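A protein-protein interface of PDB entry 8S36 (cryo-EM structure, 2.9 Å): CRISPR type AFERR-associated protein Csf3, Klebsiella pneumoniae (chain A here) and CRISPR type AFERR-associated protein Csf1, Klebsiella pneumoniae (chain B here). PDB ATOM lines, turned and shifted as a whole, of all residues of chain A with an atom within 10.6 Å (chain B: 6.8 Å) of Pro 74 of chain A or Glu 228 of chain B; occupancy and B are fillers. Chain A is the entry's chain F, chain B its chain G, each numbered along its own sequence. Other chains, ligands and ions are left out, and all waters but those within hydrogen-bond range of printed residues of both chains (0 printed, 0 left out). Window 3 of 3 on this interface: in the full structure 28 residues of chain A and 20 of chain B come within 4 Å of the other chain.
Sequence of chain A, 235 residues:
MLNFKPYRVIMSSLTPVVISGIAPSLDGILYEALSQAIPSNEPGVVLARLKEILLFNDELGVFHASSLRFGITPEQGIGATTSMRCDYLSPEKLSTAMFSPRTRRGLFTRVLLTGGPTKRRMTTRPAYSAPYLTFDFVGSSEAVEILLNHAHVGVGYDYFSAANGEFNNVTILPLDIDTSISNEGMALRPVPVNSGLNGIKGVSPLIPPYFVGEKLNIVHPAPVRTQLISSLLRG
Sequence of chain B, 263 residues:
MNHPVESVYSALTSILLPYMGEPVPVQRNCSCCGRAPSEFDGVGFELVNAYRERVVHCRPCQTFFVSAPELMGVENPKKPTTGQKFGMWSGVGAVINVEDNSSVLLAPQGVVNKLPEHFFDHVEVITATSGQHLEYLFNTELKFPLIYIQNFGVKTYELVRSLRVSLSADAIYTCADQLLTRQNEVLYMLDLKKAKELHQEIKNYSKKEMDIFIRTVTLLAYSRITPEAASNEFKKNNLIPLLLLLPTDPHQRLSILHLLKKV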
ATOM      1  N   PHE A  70      34.529  33.594 -11.552  1.00  0.00           N
ATOM      2  CA  PHE A  70      33.882  33.348 -12.829  1.00  0.00           C
ATOM      3  C   PHE A  70      32.613  32.530 -12.621  1.00  0.00           C
ATOM      4  O   PHE A  70      32.639  31.471 -11.991  1.00  0.00           O
ATOM      5  CB  PHE A  70      34.834  32.621 -13.774  1.00  0.00           C
ATOM      6  CG  PHE A  70      36.064  33.410 -14.113  1.00  0.00           C
ATOM      7  CD1 PHE A  70      36.032  34.376 -15.104  1.00  0.00           C
ATOM      8  CD2 PHE A  70      37.253  33.183 -13.445  1.00  0.00           C
ATOM      9  CE1 PHE A  70      37.163  35.101 -15.418  1.00  0.00           C
ATOM     10  CE2 PHE A  70      38.386  33.906 -13.755  1.00  0.00           C
ATOM     11  CZ  PHE A  70      38.342  34.865 -14.744  1.00  0.00           C
ATOM     12  N   GLY A  71      31.511  33.016 -13.178  1.00  0.00           N
ATOM     13  CA  GLY A  71      30.263  32.291 -13.190  1.00  0.00           C
ATOM     14  C   GLY A  71      30.155  31.490 -14.466  1.00  0.00           C
ATOM     15  O   GLY A  71      30.036  32.054 -15.566  1.00  0.00           O
ATOM     16  N   ILE A  72      30.230  30.169 -14.317  1.00  0.00           N
ATOM     17  CA  ILE A  72      30.225  29.227 -15.429  1.00  0.00           C
ATOM     18  C   ILE A  72      28.877  28.522 -15.455  1.00  0.00           C
ATOM     19  O   ILE A  72      28.385  28.067 -14.417  1.00  0.00           O
ATOM     20  CB  ILE A  72      31.378  28.213 -15.313  1.00  0.00           C
ATOM     21  CG1 ILE A  72      31.436  27.602 -13.908  1.00  0.00           C
ATOM     22  CG2 ILE A  72      32.701  28.882 -15.641  1.00  0.00           C
ATOM     23  CD1 ILE A  72      32.309  26.374 -13.812  1.00  0.00           C
ATOM     24  N   THR A  73      28.283  28.449 -16.630  1.00  0.00           N
ATOM     25  CA  THR A  73      27.005  27.799 -16.855  1.00  0.00           C
ATOM     26  C   THR A  73      27.209  26.384 -17.375  1.00  0.00           C
ATOM     27  O   THR A  73      28.311  26.008 -17.782  1.00  0.00           O
ATOM     28  CB  THR A  73      26.178  28.622 -17.840  1.00  0.00           C
ATOM     29  OG1 THR A  73      26.744  28.516 -19.152  1.00  0.00           O
ATOM     30  CG2 THR A  73      26.169  30.069 -17.413  1.00  0.00           C
ATOM     31  N   PRO A  74      26.157  25.561 -17.385  1.00  0.00           N
ATOM     32  CA  PRO A  74      26.303  24.209 -17.952  1.00  0.00           C
ATOM     33  C   PRO A  74      26.600  24.199 -19.442  1.00  0.00           C
ATOM     34  O   PRO A  74      27.049  23.167 -19.955  1.00  0.00           O
ATOM     35  CB  PRO A  74      24.951  23.544 -17.647  1.00  0.00           C
ATOM     36  CG  PRO A  74      24.038  24.639 -17.216  1.00  0.00           C
ATOM     37  CD  PRO A  74      24.895  25.709 -16.644  1.00  0.00           C
ATOM     38  N   GLU A  75      26.369  25.304 -20.149  1.00  0.00           N
ATOM     39  CA  GLU A  75      26.660  25.387 -21.577  1.00  0.00           C
ATOM     40  C   GLU A  75      28.073  25.904 -21.831  1.00  0.00           C
ATOM     41  O   GLU A  75      28.799  25.332 -22.651  1.00  0.00           O
ATOM     42  CB  GLU A  75      25.626  26.239 -22.342  1.00  0.00           C
ATOM     43  CG  GLU A  75      25.210  27.609 -21.778  1.00  0.00           C
ATOM     44  CD  GLU A  75      24.359  27.527 -20.522  1.00  0.00           C
ATOM     45  OE1 GLU A  75      24.732  26.789 -19.589  1.00  0.00           O
ATOM     46  OE2 GLU A  75      23.307  28.199 -20.472  1.00  0.00           O
ATOM     47  N   GLN A  76      28.482  26.971 -21.148  1.00  0.00           N
ATOM     48  CA  GLN A  76      29.806  27.556 -21.319  1.00  0.00           C
ATOM     49  C   GLN A  76      30.518  27.622 -19.977  1.00  0.00           C
ATOM     50  O   GLN A  76      29.924  28.008 -18.965  1.00  0.00           O
ATOM     51  CB  GLN A  76      29.722  28.962 -21.922  1.00  0.00           C
ATOM     52  CG  GLN A  76      31.063  29.512 -22.390  1.00  0.00           C
ATOM     53  CD  GLN A  76      30.962  30.929 -22.917  1.00  0.00           C
ATOM     54  OE1 GLN A  76      29.910  31.353 -23.394  1.00  0.00           O
ATOM     55  NE2 GLN A  76      32.060  31.673 -22.829  1.00  0.00           N
ATOM     56  N   GLY A  77      31.789  27.224 -19.976  1.00  0.00           N
ATOM     57  CA  GLY A  77      32.604  27.229 -18.777  1.00  0.00           C
ATOM     58  C   GLY A  77      33.867  28.050 -18.923  1.00  0.00           C
ATOM     59  O   GLY A  77      34.062  28.732 -19.933  1.00  0.00           O
ATOM     60  N   ILE A  78      34.738  27.986 -17.917  1.00  0.00           N
ATOM     61  CA  ILE A  78      35.987  28.736 -17.953  1.00  0.00           C
ATOM     62  C   ILE A  78      36.873  28.169 -19.053  1.00  0.00           C
ATOM     63  O   ILE A  78      37.088  26.953 -19.137  1.00  0.00           O
ATOM     64  CB  ILE A  78      36.679  28.689 -16.582  1.00  0.00           C
ATOM     65  CG1 ILE A  78      37.794  29.735 -16.501  1.00  0.00           C
ATOM     66  CG2 ILE A  78      37.248  27.305 -16.304  1.00  0.00           C
ATOM     67  CD1 ILE A  78      37.306  31.125 -16.185  1.00  0.00           C
ATOM     68  N   ALA A 130      35.086  33.003 -19.450  1.00  0.00           N
ATOM     69  CA  ALA A 130      33.929  32.377 -18.843  1.00  0.00           C
ATOM     70  C   ALA A 130      32.682  33.197 -19.144  1.00  0.00           C
ATOM     71  O   ALA A 130      32.769  34.414 -19.324  1.00  0.00           O
ATOM     72  CB  ALA A 130      34.093  32.250 -17.325  1.00  0.00           C
ATOM     73  N   PRO A 131      31.507  32.567 -19.215  1.00  0.00           N
ATOM     74  CA  PRO A 131      30.316  33.316 -19.640  1.00  0.00           C
ATOM     75  C   PRO A 131      29.966  34.482 -18.731  1.00  0.00           C
ATOM     76  O   PRO A 131      29.415  35.477 -19.218  1.00  0.00           O
ATOM     77  CB  PRO A 131      29.215  32.248 -19.653  1.00  0.00           C
ATOM     78  CG  PRO A 131      29.689  31.192 -18.744  1.00  0.00           C
ATOM     79  CD  PRO A 131      31.181  31.176 -18.858  1.00  0.00           C
ATOM     80  N   TYR A 132      30.260  34.399 -17.433  1.00  0.00           N
ATOM     81  CA  TYR A 132      29.869  35.448 -16.500  1.00  0.00           C
ATOM     82  C   TYR A 132      31.009  35.756 -15.544  1.00  0.00           C
ATOM     83  O   TYR A 132      31.825  34.893 -15.230  1.00  0.00           O
ATOM     84  CB  TYR A 132      28.612  35.055 -15.722  1.00  0.00           C
ATOM     85  CG  TYR A 132      27.449  34.820 -16.641  1.00  0.00           C
ATOM     86  CD1 TYR A 132      26.692  35.879 -17.117  1.00  0.00           C
ATOM     87  CD2 TYR A 132      27.133  33.544 -17.070  1.00  0.00           C
ATOM     88  CE1 TYR A 132      25.637  35.667 -17.974  1.00  0.00           C
ATOM     89  CE2 TYR A 132      26.084  33.325 -17.925  1.00  0.00           C
ATOM     90  CZ  TYR A 132      25.344  34.384 -18.378  1.00  0.00           C
ATOM     91  OH  TYR A 132      24.299  34.146 -19.229  1.00  0.00           O
ATOM     92  N   GLN A 227      32.293  29.264 -10.156  1.00  0.00           N
ATOM     93  CA  GLN A 227      31.083  28.809  -9.491  1.00  0.00           C
ATOM     94  C   GLN A 227      29.987  28.642 -10.532  1.00  0.00           C
ATOM     95  O   GLN A 227      29.948  29.362 -11.534  1.00  0.00           O
ATOM     96  CB  GLN A 227      30.636  29.799  -8.406  1.00  0.00           C
ATOM     97  CG  GLN A 227      29.593  29.256  -7.443  1.00  0.00           C
ATOM     98  CD  GLN A 227      30.195  28.373  -6.371  1.00  0.00           C
ATOM     99  OE1 GLN A 227      30.106  27.148  -6.439  1.00  0.00           O
ATOM    100  NE2 GLN A 227      30.812  28.992  -5.372  1.00  0.00           N
ATOM    101  N   LEU A 228      29.092  27.689 -10.286  1.00  0.00           N
ATOM    102  CA  LEU A 228      27.922  27.545 -11.140  1.00  0.00           C
ATOM    103  C   LEU A 228      27.058  28.794 -11.047  1.00  0.00           C
ATOM    104  O   LEU A 228      26.889  29.374  -9.971  1.00  0.00           O
ATOM    105  CB  LEU A 228      27.113  26.309 -10.741  1.00  0.00           C
ATOM    106  CG  LEU A 228      27.343  25.032 -11.556  1.00  0.00           C
ATOM    107  CD1 LEU A 228      26.974  25.233 -13.022  1.00  0.00           C
ATOM    108  CD2 LEU A 228      28.782  24.549 -11.425  1.00  0.00           C
ATOM    109  N   ILE A 229      26.502  29.211 -12.188  1.00  0.00           N
ATOM    110  CA  ILE A 229      25.665  30.405 -12.194  1.00  0.00           C
ATOM    111  C   ILE A 229      24.431  30.198 -11.328  1.00  0.00           C
ATOM    112  O   ILE A 229      23.928  31.146 -10.711  1.00  0.00           O
ATOM    113  CB  ILE A 229      25.294  30.777 -13.645  1.00  0.00           C
ATOM    114  CG1 ILE A 229      24.874  32.244 -13.738  1.00  0.00           C
ATOM    115  CG2 ILE A 229      24.186  29.876 -14.171  1.00  0.00           C
ATOM    116  CD1 ILE A 229      26.032  33.217 -13.671  1.00  0.00           C
ATOM    117  N   SER A 230      23.936  28.960 -11.246  1.00  0.00           N
ATOM    118  CA  SER A 230      22.815  28.672 -10.358  1.00  0.00           C
ATOM    119  C   SER A 230      23.195  28.916  -8.904  1.00  0.00           C
ATOM    120  O   SER A 230      22.420  29.505  -8.140  1.00  0.00           O
ATOM    121  CB  SER A 230      22.351  27.231 -10.556  1.00  0.00           C
ATOM    122  OG  SER A 230      23.455  26.347 -10.633  1.00  0.00           O
ATOM    123  N   SER A 231      24.392  28.482  -8.506  1.00  0.00           N
ATOM    124  CA  SER A 231      24.823  28.678  -7.128  1.00  0.00           C
ATOM    125  C   SER A 231      25.076  30.149  -6.831  1.00  0.00           C
ATOM    126  O   SER A 231      24.883  30.591  -5.694  1.00  0.00           O
ATOM    127  CB  SER A 231      26.083  27.858  -6.851  1.00  0.00           C
ATOM    128  OG  SER A 231      25.775  26.481  -6.728  1.00  0.00           O
ATOM    129  N   LEU A 232      25.501  30.917  -7.834  1.00  0.00           N
ATOM    130  CA  LEU A 232      25.711  32.342  -7.623  1.00  0.00           C
ATOM    131  C   LEU A 232      24.383  33.078  -7.505  1.00  0.00           C
ATOM    132  O   LEU A 232      24.258  34.018  -6.712  1.00  0.00           O
ATOM    133  CB  LEU A 232      26.545  32.920  -8.764  1.00  0.00           C
ATOM    134  CG  LEU A 232      27.960  32.352  -8.887  1.00  0.00           C
ATOM    135  CD1 LEU A 232      28.583  32.767 -10.210  1.00  0.00           C
ATOM    136  CD2 LEU A 232      28.817  32.791  -7.707  1.00  0.00           C
ATOM    137  N   LEU A 233      23.382  32.666  -8.282  1.00  0.00           N
ATOM    138  CA  LEU A 233      22.067  33.288  -8.197  1.00  0.00           C
ATOM    139  C   LEU A 233      21.232  32.758  -7.041  1.00  0.00           C
ATOM    140  O   LEU A 233      20.170  33.322  -6.760  1.00  0.00           O
ATOM    141  CB  LEU A 233      21.302  33.088  -9.505  1.00  0.00           C
ATOM    142  CG  LEU A 233      21.529  34.172 -10.558  1.00  0.00           C
ATOM    143  CD1 LEU A 233      23.000  34.309 -10.895  1.00  0.00           C
ATOM    144  CD2 LEU A 233      20.737  33.864 -11.799  1.00  0.00           C
ATOM    145  N   LEU B 220      37.417  21.096 -22.517  1.00  0.00           N
ATOM    146  CA  LEU B 220      36.743  22.053 -21.648  1.00  0.00           C
ATOM    147  C   LEU B 220      37.587  23.305 -21.456  1.00  0.00           C
ATOM    148  O   LEU B 220      37.067  24.426 -21.490  1.00  0.00           O
ATOM    149  CB  LEU B 220      36.432  21.400 -20.302  1.00  0.00           C
ATOM    150  CG  LEU B 220      35.599  22.209 -19.307  1.00  0.00           C
ATOM    151  CD1 LEU B 220      34.266  22.632 -19.909  1.00  0.00           C
ATOM    152  CD2 LEU B 220      35.383  21.398 -18.041  1.00  0.00           C
ATOM    153  N   ILE B 225      33.815  21.719 -25.375  1.00  0.00           N
ATOM    154  CA  ILE B 225      32.699  20.938 -24.859  1.00  0.00           C
ATOM    155  C   ILE B 225      32.043  21.727 -23.739  1.00  0.00           C
ATOM    156  O   ILE B 225      32.721  22.431 -22.982  1.00  0.00           O
ATOM    157  CB  ILE B 225      33.152  19.550 -24.358  1.00  0.00           C
ATOM    158  CG1 ILE B 225      34.284  19.684 -23.336  1.00  0.00           C
ATOM    159  CG2 ILE B 225      33.589  18.687 -25.530  1.00  0.00           C
ATOM    160  CD1 ILE B 225      34.685  18.375 -22.705  1.00  0.00           C
ATOM    161  N   THR B 226      30.726  21.609 -23.634  1.00  0.00           N
ATOM    162  CA  THR B 226      30.012  22.295 -22.575  1.00  0.00           C
ATOM    163  C   THR B 226      30.398  21.702 -21.219  1.00  0.00           C
ATOM    164  O   THR B 226      30.714  20.514 -21.123  1.00  0.00           O
ATOM    165  CB  THR B 226      28.505  22.179 -22.778  1.00  0.00           C
ATOM    166  OG1 THR B 226      28.095  20.822 -22.576  1.00  0.00           O
ATOM    167  CG2 THR B 226      28.112  22.628 -24.179  1.00  0.00           C
ATOM    168  N   PRO B 227      30.390  22.510 -20.152  1.00  0.00           N
ATOM    169  CA  PRO B 227      30.657  21.940 -18.822  1.00  0.00           C
ATOM    170  C   PRO B 227      29.707  20.822 -18.449  1.00  0.00           C
ATOM    171  O   PRO B 227      30.109  19.893 -17.740  1.00  0.00           O
ATOM    172  CB  PRO B 227      30.506  23.151 -17.892  1.00  0.00           C
ATOM    173  CG  PRO B 227      30.867  24.297 -18.743  1.00  0.00           C
ATOM    174  CD  PRO B 227      30.286  23.978 -20.088  1.00  0.00           C
ATOM    175  N   GLU B 228      28.453  20.884 -18.898  1.00  0.00           N
ATOM    176  CA  GLU B 228      27.515  19.803 -18.618  1.00  0.00           C
ATOM    177  C   GLU B 228      27.987  18.501 -19.253  1.00  0.00           C
ATOM    178  O   GLU B 228      27.990  17.446 -18.607  1.00  0.00           O
ATOM    179  CB  GLU B 228      26.122  20.179 -19.123  1.00  0.00           C
ATOM    180  CG  GLU B 228      25.008  19.259 -18.637  1.00  0.00           C
ATOM    181  CD  GLU B 228      23.801  19.240 -19.560  1.00  0.00           C
ATOM    182  OE1 GLU B 228      23.824  19.927 -20.603  1.00  0.00           O
ATOM    183  OE2 GLU B 228      22.822  18.534 -19.238  1.00  0.00           O
ATOM    184  N   ALA B 229      28.389  18.556 -20.524  1.00  0.00           N
ATOM    185  CA  ALA B 229      28.877  17.356 -21.195  1.00  0.00           C
ATOM    186  C   ALA B 229      30.139  16.826 -20.527  1.00  0.00           C
ATOM    187  O   ALA B 229      30.288  15.612 -20.337  1.00  0.00           O
ATOM    188  CB  ALA B 229      29.138  17.652 -22.670  1.00  0.00           C
ATOM    189  N   ALA B 230      31.065  17.719 -20.172  1.00  0.00           N
ATOM    190  CA  ALA B 230      32.293  17.279 -19.520  1.00  0.00           C
ATOM    191  C   ALA B 230      31.997  16.629 -18.177  1.00  0.00           C
ATOM    192  O   ALA B 230      32.581  15.595 -17.837  1.00  0.00           O
ATOM    193  CB  ALA B 230      33.245  18.460 -19.344  1.00  0.00           C
ATOM    194  N   SER B 231      31.070  17.207 -17.411  1.00  0.00           N
ATOM    195  CA  SER B 231      30.703  16.619 -16.128  1.00  0.00           C
ATOM    196  C   SER B 231      30.049  15.261 -16.324  1.00  0.00           C
ATOM    197  O   SER B 231      30.286  14.330 -15.546  1.00  0.00           O
ATOM    198  CB  SER B 231      29.770  17.560 -15.369  1.00  0.00           C
ATOM    199  OG  SER B 231      28.465  17.533 -15.920  1.00  0.00           O
ATOM    200  N   ASN B 232      29.216  15.131 -17.358  1.00  0.00           N
ATOM    201  CA  ASN B 232      28.612  13.838 -17.655  1.00  0.00           C
ATOM    202  C   ASN B 232      29.678  12.798 -17.966  1.00  0.00           C
ATOM    203  O   ASN B 232      29.617  11.669 -17.469  1.00  0.00           O
ATOM    204  CB  ASN B 232      27.639  13.972 -18.826  1.00  0.00           C
ATOM    205  CG  ASN B 232      26.383  14.732 -18.454  1.00  0.00           C
ATOM    206  OD1 ASN B 232      26.322  15.379 -17.408  1.00  0.00           O
ATOM    207  ND2 ASN B 232      25.371  14.658 -19.310  1.00  0.00           N
ATOM    208  N   GLU B 233      30.667  13.163 -18.786  1.00  0.00           N
ATOM    209  CA  GLU B 233      31.739  12.223 -19.107  1.00  0.00           C
ATOM    210  C   GLU B 233      32.530  11.847 -17.860  1.00  0.00           C
ATOM    211  O   GLU B 233      32.852  10.672 -17.650  1.00  0.00           O
ATOM    212  CB  GLU B 233      32.674  12.818 -20.164  1.00  0.00           C
ATOM    213  CG  GLU B 233      32.022  13.221 -21.490  1.00  0.00           C
ATOM    214  CD  GLU B 233      30.701  12.523 -21.757  1.00  0.00           C
ATOM    215  OE1 GLU B 233      30.699  11.281 -21.890  1.00  0.00           O
ATOM    216  OE2 GLU B 233      29.664  13.216 -21.831  1.00  0.00           O
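The backbone NH (N) of Glu 228 of chain B sits at hydrogen-bond distance from the backbone carbonyl oxygen (O) of Pro 74 of chain A (2.9 Å). The backbone carbonyl oxygen (O) of Pro 74 of chain A sits close to the backbone nitrogen (N) of Pro 227 of chain B (3.4 Å). The backbone carbonyl oxygen of Leu 220 of chain B sits close to the backbone carbonyl oxygen of Ile 78 of chain A, at 3.5 Å.
The side-chain hydroxyl of Thr 73 of chain A is in hydrogen-bond range of the side-chain carboxylate of Glu 75 of chain A (2.7 Å). OG1 of Thr 73 of chain A lies within hydrogen-bond range of N of Gln 76 of chain A. N of Ala 229 of chain B is in hydrogen-bond range of OG1 of Thr 226 of chain B (3.1 Å). The backbone carbonyl oxygen (O) of Pro 227 of chain B lies close to the side-chain hydroxyl (OG) of Ser 231 of chain B, 3.4 Å away. The backbone carbonyl oxygen of Glu 228 of chain B is in hydrogen-bond range of the side-chain hydroxyl of Ser 231 of chain B, 2.7 Å away. The backbone carbonyl oxygen of Glu 228 of chain B lies close to the side-chain amide oxygen of Asn 232 of chain B, 2.9 Å away.
Pro 227 of chain B touches Thr 73 of chain A. Thr 226 of chain B touches Pro 74 of chain A (CB to O, 3.3 Å). O of Glu 75 of chain A touches CB of Thr 226 of chain B, at 3.2 Å. Pro 227 of chain B touches Glu 75 of chain A. Gln 76 of chain A touches Pro 227 of chain B. N of Gly 77 of chain A touches CG of Pro 227 of chain B (3.3 Å).
Printed residues of chain B within 4 Å of Thr 73 of chain A: Pro 227. Of chain B, only Thr 226, Pro 227 and Glu 228 come within 4 Å of Pro 74 of chain A. Of the printed residues of chain B, Glu 75 of chain A touches Thr 226 (3.2 Å) and Pro 227 (3.3 Å). Printed residues of chain B within 4 Å of Ile 78 of chain A: Leu 220 (3.5 Å). Printed residues of chain A within 4 Å of Leu 220 of chain B: Ile 78. Pro 227 of chain B touches five residues of chain A. Glu 228 of chain B touches just one residue of chain A: Pro 74. No residue of chain A comes within 4 Å of Ala 229 of chain B. No residue of chain A comes within 4 Å of Ala 230 of chain B. No residue of chain A comes within 4 Å of Ser 231 of chain B. No residue of chain A comes within 4 Å of Asn 232 of chain B. The nearest residue of chain B that does not touch Pro 74 of chain A is Ala 229 of chain B (4.8 Å).
Along chain A the printed residues that touch a printed residue of chain B span positions 73 to 78. Of the 10 printed residues of chain B, 4 touch a printed residue of chain A. Hydrophobic or aromatic side chains of chain B that line the printed part of chain A: Pro 227. Along chain B the printed residues that touch a printed residue of chain A span positions 220 to 228. Among the printed residues, 9 pairs touch across the chains. Among the printed residues, no Asp or Glu carboxylate lies within 4 Å of a Lys or Arg side-chain nitrogen of the other chain.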
